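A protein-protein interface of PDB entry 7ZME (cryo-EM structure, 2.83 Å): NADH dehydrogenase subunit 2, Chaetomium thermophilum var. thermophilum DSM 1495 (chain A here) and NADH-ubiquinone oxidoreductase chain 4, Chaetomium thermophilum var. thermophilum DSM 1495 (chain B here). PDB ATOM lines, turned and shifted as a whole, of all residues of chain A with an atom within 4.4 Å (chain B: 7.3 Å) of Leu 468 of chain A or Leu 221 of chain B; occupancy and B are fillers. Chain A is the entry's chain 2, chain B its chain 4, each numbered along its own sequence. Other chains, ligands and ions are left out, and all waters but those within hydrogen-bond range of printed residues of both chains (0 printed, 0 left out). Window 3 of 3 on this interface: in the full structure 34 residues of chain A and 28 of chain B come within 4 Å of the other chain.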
ATOM      1  N   LEU A 459       2.566 -32.277  -2.960  1.00  0.00           N
ATOM      2  CA  LEU A 459       1.861 -31.052  -2.503  1.00  0.00           C
ATOM      3  C   LEU A 459       1.122 -31.358  -1.203  1.00  0.00           C
ATOM      4  O   LEU A 459       1.206 -30.542  -0.276  1.00  0.00           O
ATOM      5  CB  LEU A 459       0.884 -30.588  -3.584  1.00  0.00           C
ATOM      6  CG  LEU A 459       1.445 -29.681  -4.674  1.00  0.00           C
ATOM      7  CD1 LEU A 459       0.390 -29.429  -5.736  1.00  0.00           C
ATOM      8  CD2 LEU A 459       1.936 -28.368  -4.094  1.00  0.00           C
ATOM      9  N   ILE A 464       6.432 -28.697  -0.706  1.00  0.00           N
ATOM     10  CA  ILE A 464       6.041 -27.629  -1.667  1.00  0.00           C
ATOM     11  C   ILE A 464       7.278 -27.169  -2.423  1.00  0.00           C
ATOM     12  O   ILE A 464       7.155 -26.880  -3.614  1.00  0.00           O
ATOM     13  CB  ILE A 464       5.377 -26.461  -0.910  1.00  0.00           C
ATOM     14  CG1 ILE A 464       4.342 -26.957   0.103  1.00  0.00           C
ATOM     15  CG2 ILE A 464       4.781 -25.447  -1.874  1.00  0.00           C
ATOM     16  CD1 ILE A 464       3.173 -27.680  -0.519  1.00  0.00           C
ATOM     17  N   PHE A 465       8.417 -27.103  -1.739  1.00  0.00           N
ATOM     18  CA  PHE A 465       9.601 -26.556  -2.393  1.00  0.00           C
ATOM     19  C   PHE A 465      10.092 -27.469  -3.511  1.00  0.00           C
ATOM     20  O   PHE A 465      10.480 -26.992  -4.582  1.00  0.00           O
ATOM     21  CB  PHE A 465      10.692 -26.311  -1.349  1.00  0.00           C
ATOM     22  CG  PHE A 465      11.948 -25.712  -1.901  1.00  0.00           C
ATOM     23  CD1 PHE A 465      12.056 -24.346  -2.079  1.00  0.00           C
ATOM     24  CD2 PHE A 465      13.031 -26.511  -2.219  1.00  0.00           C
ATOM     25  CE1 PHE A 465      13.212 -23.792  -2.580  1.00  0.00           C
ATOM     26  CE2 PHE A 465      14.187 -25.961  -2.720  1.00  0.00           C
ATOM     27  CZ  PHE A 465      14.279 -24.600  -2.900  1.00  0.00           C
ATOM     28  N   LEU A 466      10.082 -28.786  -3.284  1.00  0.00           N
ATOM     29  CA  LEU A 466      10.457 -29.723  -4.341  1.00  0.00           C
ATOM     30  C   LEU A 466       9.438 -29.753  -5.469  1.00  0.00           C
ATOM     31  O   LEU A 466       9.795 -30.057  -6.610  1.00  0.00           O
ATOM     32  CB  LEU A 466      10.649 -31.131  -3.775  1.00  0.00           C
ATOM     33  CG  LEU A 466      11.987 -31.511  -3.135  1.00  0.00           C
ATOM     34  CD1 LEU A 466      13.086 -31.467  -4.171  1.00  0.00           C
ATOM     35  CD2 LEU A 466      12.337 -30.612  -1.970  1.00  0.00           C
ATOM     36  N   SER A 467       8.171 -29.464  -5.173  1.00  0.00           N
ATOM     37  CA  SER A 467       7.177 -29.368  -6.235  1.00  0.00           C
ATOM     38  C   SER A 467       7.434 -28.155  -7.117  1.00  0.00           C
ATOM     39  O   SER A 467       7.268 -28.221  -8.338  1.00  0.00           O
ATOM     40  CB  SER A 467       5.774 -29.313  -5.638  1.00  0.00           C
ATOM     41  OG  SER A 467       5.397 -30.568  -5.111  1.00  0.00           O
ATOM     42  N   LEU A 468       7.828 -27.034  -6.509  1.00  0.00           N
ATOM     43  CA  LEU A 468       8.179 -25.853  -7.285  1.00  0.00           C
ATOM     44  C   LEU A 468       9.418 -26.098  -8.133  1.00  0.00           C
ATOM     45  O   LEU A 468       9.470 -25.694  -9.297  1.00  0.00           O
ATOM     46  CB  LEU A 468       8.392 -24.664  -6.354  1.00  0.00           C
ATOM     47  CG  LEU A 468       7.145 -24.176  -5.625  1.00  0.00           C
ATOM     48  CD1 LEU A 468       7.512 -23.121  -4.599  1.00  0.00           C
ATOM     49  CD2 LEU A 468       6.123 -23.647  -6.615  1.00  0.00           C
ATOM     50  N   ILE A 469      10.427 -26.759  -7.564  1.00  0.00           N
ATOM     51  CA  ILE A 469      11.620 -27.104  -8.332  1.00  0.00           C
ATOM     52  C   ILE A 469      11.250 -27.976  -9.520  1.00  0.00           C
ATOM     53  O   ILE A 469      11.710 -27.746 -10.644  1.00  0.00           O
ATOM     54  CB  ILE A 469      12.658 -27.800  -7.430  1.00  0.00           C
ATOM     55  CG1 ILE A 469      13.121 -26.870  -6.307  1.00  0.00           C
ATOM     56  CG2 ILE A 469      13.840 -28.283  -8.250  1.00  0.00           C
ATOM     57  CD1 ILE A 469      13.814 -25.633  -6.790  1.00  0.00           C
ATOM     58  N   ALA A 470      10.403 -28.983  -9.294  1.00  0.00           N
ATOM     59  CA  ALA A 470      10.082 -29.943 -10.345  1.00  0.00           C
ATOM     60  C   ALA A 470       9.375 -29.279 -11.519  1.00  0.00           C
ATOM     61  O   ALA A 470       9.663 -29.593 -12.678  1.00  0.00           O
ATOM     62  CB  ALA A 470       9.230 -31.076  -9.775  1.00  0.00           C
ATOM     63  N   ILE A 471       8.438 -28.367 -11.246  1.00  0.00           N
ATOM     64  CA  ILE A 471       7.713 -27.735 -12.344  1.00  0.00           C
ATOM     65  C   ILE A 471       8.613 -26.778 -13.112  1.00  0.00           C
ATOM     66  O   ILE A 471       8.468 -26.627 -14.330  1.00  0.00           O
ATOM     67  CB  ILE A 471       6.431 -27.038 -11.844  1.00  0.00           C
ATOM     68  CG1 ILE A 471       6.747 -25.881 -10.898  1.00  0.00           C
ATOM     69  CG2 ILE A 471       5.497 -28.038 -11.185  1.00  0.00           C
ATOM     70  CD1 ILE A 471       5.553 -24.992 -10.616  1.00  0.00           C
ATOM     71  N   ILE A 472       9.550 -26.117 -12.430  1.00  0.00           N
ATOM     72  CA  ILE A 472      10.464 -25.215 -13.122  1.00  0.00           C
ATOM     73  C   ILE A 472      11.439 -25.999 -13.989  1.00  0.00           C
ATOM     74  O   ILE A 472      11.739 -25.603 -15.120  1.00  0.00           O
ATOM     75  CB  ILE A 472      11.197 -24.311 -12.112  1.00  0.00           C
ATOM     76  CG1 ILE A 472      10.194 -23.489 -11.310  1.00  0.00           C
ATOM     77  CG2 ILE A 472      12.178 -23.394 -12.821  1.00  0.00           C
ATOM     78  CD1 ILE A 472       9.352 -22.568 -12.152  1.00  0.00           C
ATOM     79  N   TYR B 179      -8.152 -28.149 -17.094  1.00  0.00           N
ATOM     80  CA  TYR B 179      -6.720 -28.009 -17.328  1.00  0.00           C
ATOM     81  C   TYR B 179      -6.228 -29.003 -18.374  1.00  0.00           C
ATOM     82  O   TYR B 179      -5.292 -28.711 -19.125  1.00  0.00           O
ATOM     83  CB  TYR B 179      -5.970 -28.187 -16.008  1.00  0.00           C
ATOM     84  CG  TYR B 179      -4.463 -28.149 -16.117  1.00  0.00           C
ATOM     85  CD1 TYR B 179      -3.738 -29.294 -16.410  1.00  0.00           C
ATOM     86  CD2 TYR B 179      -3.766 -26.968 -15.922  1.00  0.00           C
ATOM     87  CE1 TYR B 179      -2.371 -29.261 -16.515  1.00  0.00           C
ATOM     88  CE2 TYR B 179      -2.397 -26.931 -16.022  1.00  0.00           C
ATOM     89  CZ  TYR B 179      -1.705 -28.080 -16.316  1.00  0.00           C
ATOM     90  OH  TYR B 179      -0.337 -28.046 -16.415  1.00  0.00           O
ATOM     91  N   GLY B 215       3.185 -21.163 -17.127  1.00  0.00           N
ATOM     92  CA  GLY B 215       2.086 -20.536 -16.377  1.00  0.00           C
ATOM     93  C   GLY B 215       1.116 -21.599 -15.920  1.00  0.00           C
ATOM     94  O   GLY B 215       0.641 -21.509 -14.786  1.00  0.00           O
ATOM     95  N   SER B 216       0.875 -22.595 -16.771  1.00  0.00           N
ATOM     96  CA  SER B 216      -0.090 -23.673 -16.459  1.00  0.00           C
ATOM     97  C   SER B 216       0.380 -24.506 -15.267  1.00  0.00           C
ATOM     98  O   SER B 216      -0.479 -24.922 -14.495  1.00  0.00           O
ATOM     99  CB  SER B 216      -0.297 -24.530 -17.656  1.00  0.00           C
ATOM    100  OG  SER B 216       0.758 -25.467 -17.798  1.00  0.00           O
ATOM    101  N   LEU B 217       1.665 -24.744 -15.113  1.00  0.00           N
ATOM    102  CA  LEU B 217       2.176 -25.615 -14.033  1.00  0.00           C
ATOM    103  C   LEU B 217       1.905 -24.923 -12.708  1.00  0.00           C
ATOM    104  O   LEU B 217       1.730 -25.626 -11.705  1.00  0.00           O
ATOM    105  CB  LEU B 217       3.632 -25.986 -14.306  1.00  0.00           C
ATOM    106  CG  LEU B 217       3.830 -26.927 -15.492  1.00  0.00           C
ATOM    107  CD1 LEU B 217       5.303 -27.145 -15.785  1.00  0.00           C
ATOM    108  CD2 LEU B 217       3.127 -28.252 -15.258  1.00  0.00           C
ATOM    109  N   PHE B 218       1.802 -23.599 -12.714  1.00  0.00           N
ATOM    110  CA  PHE B 218       1.383 -22.885 -11.516  1.00  0.00           C
ATOM    111  C   PHE B 218      -0.116 -23.030 -11.286  1.00  0.00           C
ATOM    112  O   PHE B 218      -0.565 -23.153 -10.141  1.00  0.00           O
ATOM    113  CB  PHE B 218       1.785 -21.419 -11.623  1.00  0.00           C
ATOM    114  CG  PHE B 218       3.245 -21.189 -11.400  1.00  0.00           C
ATOM    115  CD1 PHE B 218       3.747 -21.043 -10.118  1.00  0.00           C
ATOM    116  CD2 PHE B 218       4.121 -21.143 -12.468  1.00  0.00           C
ATOM    117  CE1 PHE B 218       5.089 -20.845  -9.911  1.00  0.00           C
ATOM    118  CE2 PHE B 218       5.460 -20.947 -12.267  1.00  0.00           C
ATOM    119  CZ  PHE B 218       5.947 -20.796 -10.985  1.00  0.00           C
ATOM    120  N   LEU B 219      -0.904 -23.022 -12.363  1.00  0.00           N
ATOM    121  CA  LEU B 219      -2.327 -23.315 -12.250  1.00  0.00           C
ATOM    122  C   LEU B 219      -2.555 -24.753 -11.811  1.00  0.00           C
ATOM    123  O   LEU B 219      -3.473 -25.033 -11.034  1.00  0.00           O
ATOM    124  CB  LEU B 219      -3.022 -23.050 -13.584  1.00  0.00           C
ATOM    125  CG  LEU B 219      -4.519 -23.320 -13.733  1.00  0.00           C
ATOM    126  CD1 LEU B 219      -5.330 -22.233 -13.070  1.00  0.00           C
ATOM    127  CD2 LEU B 219      -4.906 -23.451 -15.195  1.00  0.00           C
ATOM    128  N   LEU B 220      -1.731 -25.679 -12.308  1.00  0.00           N
ATOM    129  CA  LEU B 220      -1.880 -27.080 -11.935  1.00  0.00           C
ATOM    130  C   LEU B 220      -1.654 -27.281 -10.443  1.00  0.00           C
ATOM    131  O   LEU B 220      -2.383 -28.038  -9.798  1.00  0.00           O
ATOM    132  CB  LEU B 220      -0.916 -27.943 -12.750  1.00  0.00           C
ATOM    133  CG  LEU B 220      -0.958 -29.460 -12.539  1.00  0.00           C
ATOM    134  CD1 LEU B 220      -2.298 -30.056 -12.960  1.00  0.00           C
ATOM    135  CD2 LEU B 220       0.180 -30.124 -13.289  1.00  0.00           C
ATOM    136  N   LEU B 221      -0.653 -26.604  -9.874  1.00  0.00           N
ATOM    137  CA  LEU B 221      -0.385 -26.746  -8.446  1.00  0.00           C
ATOM    138  C   LEU B 221      -1.546 -26.240  -7.605  1.00  0.00           C
ATOM    139  O   LEU B 221      -1.784 -26.753  -6.506  1.00  0.00           O
ATOM    140  CB  LEU B 221       0.897 -26.006  -8.066  1.00  0.00           C
ATOM    141  CG  LEU B 221       2.247 -26.556  -8.535  1.00  0.00           C
ATOM    142  CD1 LEU B 221       3.358 -25.979  -7.682  1.00  0.00           C
ATOM    143  CD2 LEU B 221       2.290 -28.081  -8.523  1.00  0.00           C
ATOM    144  N   SER B 222      -2.271 -25.235  -8.097  1.00  0.00           N
ATOM    145  CA  SER B 222      -3.447 -24.744  -7.388  1.00  0.00           C
ATOM    146  C   SER B 222      -4.620 -25.705  -7.528  1.00  0.00           C
ATOM    147  O   SER B 222      -5.352 -25.950  -6.564  1.00  0.00           O
ATOM    148  CB  SER B 222      -3.830 -23.363  -7.910  1.00  0.00           C
ATOM    149  OG  SER B 222      -2.765 -22.448  -7.762  1.00  0.00           O
ATOM    150  N   ILE B 223      -4.821 -26.244  -8.729  1.00  0.00           N
ATOM    151  CA  ILE B 223      -5.921 -27.171  -8.961  1.00  0.00           C
ATOM    152  C   ILE B 223      -5.724 -28.438  -8.143  1.00  0.00           C
ATOM    153  O   ILE B 223      -6.684 -29.016  -7.619  1.00  0.00           O
ATOM    154  CB  ILE B 223      -6.041 -27.476 -10.465  1.00  0.00           C
ATOM    155  CG1 ILE B 223      -6.512 -26.234 -11.218  1.00  0.00           C
ATOM    156  CG2 ILE B 223      -6.965 -28.656 -10.718  1.00  0.00           C
ATOM    157  CD1 ILE B 223      -6.205 -26.276 -12.686  1.00  0.00           C
ATOM    158  N   LEU B 224      -4.458 -28.830  -7.997  1.00  0.00           N
ATOM    159  CA  LEU B 224      -4.156 -30.044  -7.207  1.00  0.00           C
ATOM    160  C   LEU B 224      -4.434 -29.820  -5.724  1.00  0.00           C
ATOM    161  O   LEU B 224      -4.997 -30.712  -5.093  1.00  0.00           O
ATOM    162  CB  LEU B 224      -2.738 -30.509  -7.534  1.00  0.00           C
ATOM    163  CG  LEU B 224      -2.549 -30.970  -8.977  1.00  0.00           C
ATOM    164  CD1 LEU B 224      -1.173 -31.574  -9.193  1.00  0.00           C
ATOM    165  CD2 LEU B 224      -3.646 -31.937  -9.383  1.00  0.00           C
ATOM    166  N   THR B 225      -4.079 -28.647  -5.217  1.00  0.00           N
ATOM    167  CA  THR B 225      -4.331 -28.315  -3.794  1.00  0.00           C
ATOM    168  C   THR B 225      -5.842 -28.350  -3.522  1.00  0.00           C
ATOM    169  O   THR B 225      -6.229 -28.894  -2.493  1.00  0.00           O
ATOM    170  CB  THR B 225      -3.613 -27.011  -3.431  1.00  0.00           C
ATOM    171  OG1 THR B 225      -2.211 -27.275  -3.405  1.00  0.00           O
ATOM    172  CG2 THR B 225      -4.057 -26.428  -2.107  1.00  0.00           C
ATOM    173  N   MET B 226      -6.666 -27.835  -4.434  1.00  0.00           N
ATOM    174  CA  MET B 226      -8.142 -27.871  -4.260  1.00  0.00           C
ATOM    175  C   MET B 226      -8.661 -29.305  -4.229  1.00  0.00           C
ATOM    176  O   MET B 226      -9.544 -29.582  -3.420  1.00  0.00           O
ATOM    177  CB  MET B 226      -8.851 -27.152  -5.411  1.00  0.00           C
ATOM    178  CG  MET B 226      -8.608 -25.667  -5.429  1.00  0.00           C
ATOM    179  SD  MET B 226      -9.291 -24.900  -6.908  1.00  0.00           S
ATOM    180  CE  MET B 226      -8.677 -23.232  -6.692  1.00  0.00           C
ATOM    181  N   PHE B 250      -3.186 -18.139  -1.535  1.00  0.00           N
ATOM    182  CA  PHE B 250      -2.197 -18.928  -2.254  1.00  0.00           C
ATOM    183  C   PHE B 250      -2.820 -19.688  -3.414  1.00  0.00           C
ATOM    184  O   PHE B 250      -2.117 -20.049  -4.360  1.00  0.00           O
ATOM    185  CB  PHE B 250      -1.482 -19.876  -1.295  1.00  0.00           C
ATOM    186  CG  PHE B 250      -0.598 -19.172  -0.311  1.00  0.00           C
ATOM    187  CD1 PHE B 250       0.616 -18.645  -0.715  1.00  0.00           C
ATOM    188  CD2 PHE B 250      -0.982 -19.018   1.007  1.00  0.00           C
ATOM    189  CE1 PHE B 250       1.433 -17.992   0.176  1.00  0.00           C
ATOM    190  CE2 PHE B 250      -0.168 -18.364   1.905  1.00  0.00           C
ATOM    191  CZ  PHE B 250       1.041 -17.851   1.488  1.00  0.00           C
ATOM    192  N   LEU B 251      -4.124 -19.951  -3.360  1.00  0.00           N
ATOM    193  CA  LEU B 251      -4.798 -20.498  -4.531  1.00  0.00           C
ATOM    194  C   LEU B 251      -4.962 -19.439  -5.610  1.00  0.00           C
ATOM    195  O   LEU B 251      -4.844 -19.740  -6.802  1.00  0.00           O
ATOM    196  CB  LEU B 251      -6.151 -21.082  -4.138  1.00  0.00           C
ATOM    197  CG  LEU B 251      -6.114 -22.419  -3.409  1.00  0.00           C
ATOM    198  CD1 LEU B 251      -7.516 -22.895  -3.121  1.00  0.00           C
ATOM    199  CD2 LEU B 251      -5.352 -23.439  -4.229  1.00  0.00           C
ATOM    200  N   PHE B 253      -2.963 -16.819  -6.302  1.00  0.00           N
ATOM    201  CA  PHE B 253      -1.678 -16.831  -6.978  1.00  0.00           C
ATOM    202  C   PHE B 253      -1.393 -18.228  -7.512  1.00  0.00           C
ATOM    203  O   PHE B 253      -1.748 -19.238  -6.901  1.00  0.00           O
ATOM    204  CB  PHE B 253      -0.575 -16.384  -6.025  1.00  0.00           C
ATOM    205  CG  PHE B 253      -0.838 -15.060  -5.371  1.00  0.00           C
ATOM    206  CD1 PHE B 253      -1.249 -13.974  -6.123  1.00  0.00           C
ATOM    207  CD2 PHE B 253      -0.667 -14.900  -4.008  1.00  0.00           C
ATOM    208  CE1 PHE B 253      -1.487 -12.754  -5.525  1.00  0.00           C
ATOM    209  CE2 PHE B 253      -0.903 -13.682  -3.403  1.00  0.00           C
ATOM    210  CZ  PHE B 253      -1.313 -12.608  -4.162  1.00  0.00           C
ATOM    211  N   GLY B 254      -0.745 -18.288  -8.662  1.00  0.00           N
ATOM    212  CA  GLY B 254      -0.662 -19.548  -9.368  1.00  0.00           C
ATOM    213  C   GLY B 254      -1.771 -19.655 -10.391  1.00  0.00           C
ATOM    214  O   GLY B 254      -1.498 -19.785 -11.586  1.00  0.00           O
ATOM    215  N   ILE B 255      -3.026 -19.600  -9.942  1.00  0.00           N
ATOM    216  CA  ILE B 255      -4.130 -19.452 -10.885  1.00  0.00           C
ATOM    217  C   ILE B 255      -4.020 -18.119 -11.609  1.00  0.00           C
ATOM    218  O   ILE B 255      -4.152 -18.044 -12.835  1.00  0.00           O
ATOM    219  CB  ILE B 255      -5.486 -19.584 -10.172  1.00  0.00           C
ATOM    220  CG1 ILE B 255      -5.742 -21.024  -9.746  1.00  0.00           C
ATOM    221  CG2 ILE B 255      -6.609 -19.121 -11.085  1.00  0.00           C
ATOM    222  CD1 ILE B 255      -7.020 -21.191  -8.979  1.00  0.00           C
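Printed residues of chain B within 4 Å of Leu 459 of chain A: Leu 221 and Leu 224. Leu 468 of chain A touches just one residue of chain B: Leu 221. Printed residues of chain B within 4 Å of Ile 471 of chain A: Leu 217 and Leu 221. Of the printed residues of chain A, Leu 217 of chain B touches Ile 471. Phe 218 of chain B touches none of the printed residues of chain A. Of chain A, only Leu 459, Leu 468 and Ile 471 come within 4 Å of Leu 221 of chain B. Printed residues of chain A within 4 Å of Leu 224 of chain B: Leu 459. Phe 250 of chain B touches none of the printed residues of chain A. The nearest residue of chain B that does not touch Leu 468 of chain A is Phe 218 of chain B (4.4 Å). The nearest printed residue of chain A that does not touch Leu 221 of chain B is Ser 467 of chain A (4.6 Å). The nearest printed residue of chain B that does not touch Ile 471 of chain A is Phe 218 of chain B (4.2 Å).
Of the 10 printed residues of chain A, 3 touch a printed residue of chain B. Hydrophobic or aromatic side chains of chain A that line the printed part of chain B: Leu 459, Leu 468 and Ile 471. Hydrophobic or aromatic side chains of chain B within 4 Å of the printed part of chain A: Leu 217, Leu 221 and Leu 224. Along chain B the printed residues that touch a printed residue of chain A span positions 217 to 224.
The backbone carbonyl oxygen (O) of Leu 221 of chain B is in hydrogen-bond range of the side-chain hydroxyl (OG1) of Thr 225 of chain B, 3.2 Å away.
Leu 221 of chain B touches Leu 459 of chain A. Leu 459 of chain A touches Leu 224 of chain B (CD1 to CB, 3.8 Å). Leu 468 of chain A touches Leu 221 of chain B (CD2 to CD1, 3.8 Å). Ile 471 of chain A touches Leu 217 of chain B. Leu 221 of chain B touches Ile 471 of chain A (CD1 to CD1, 3.8 Å).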
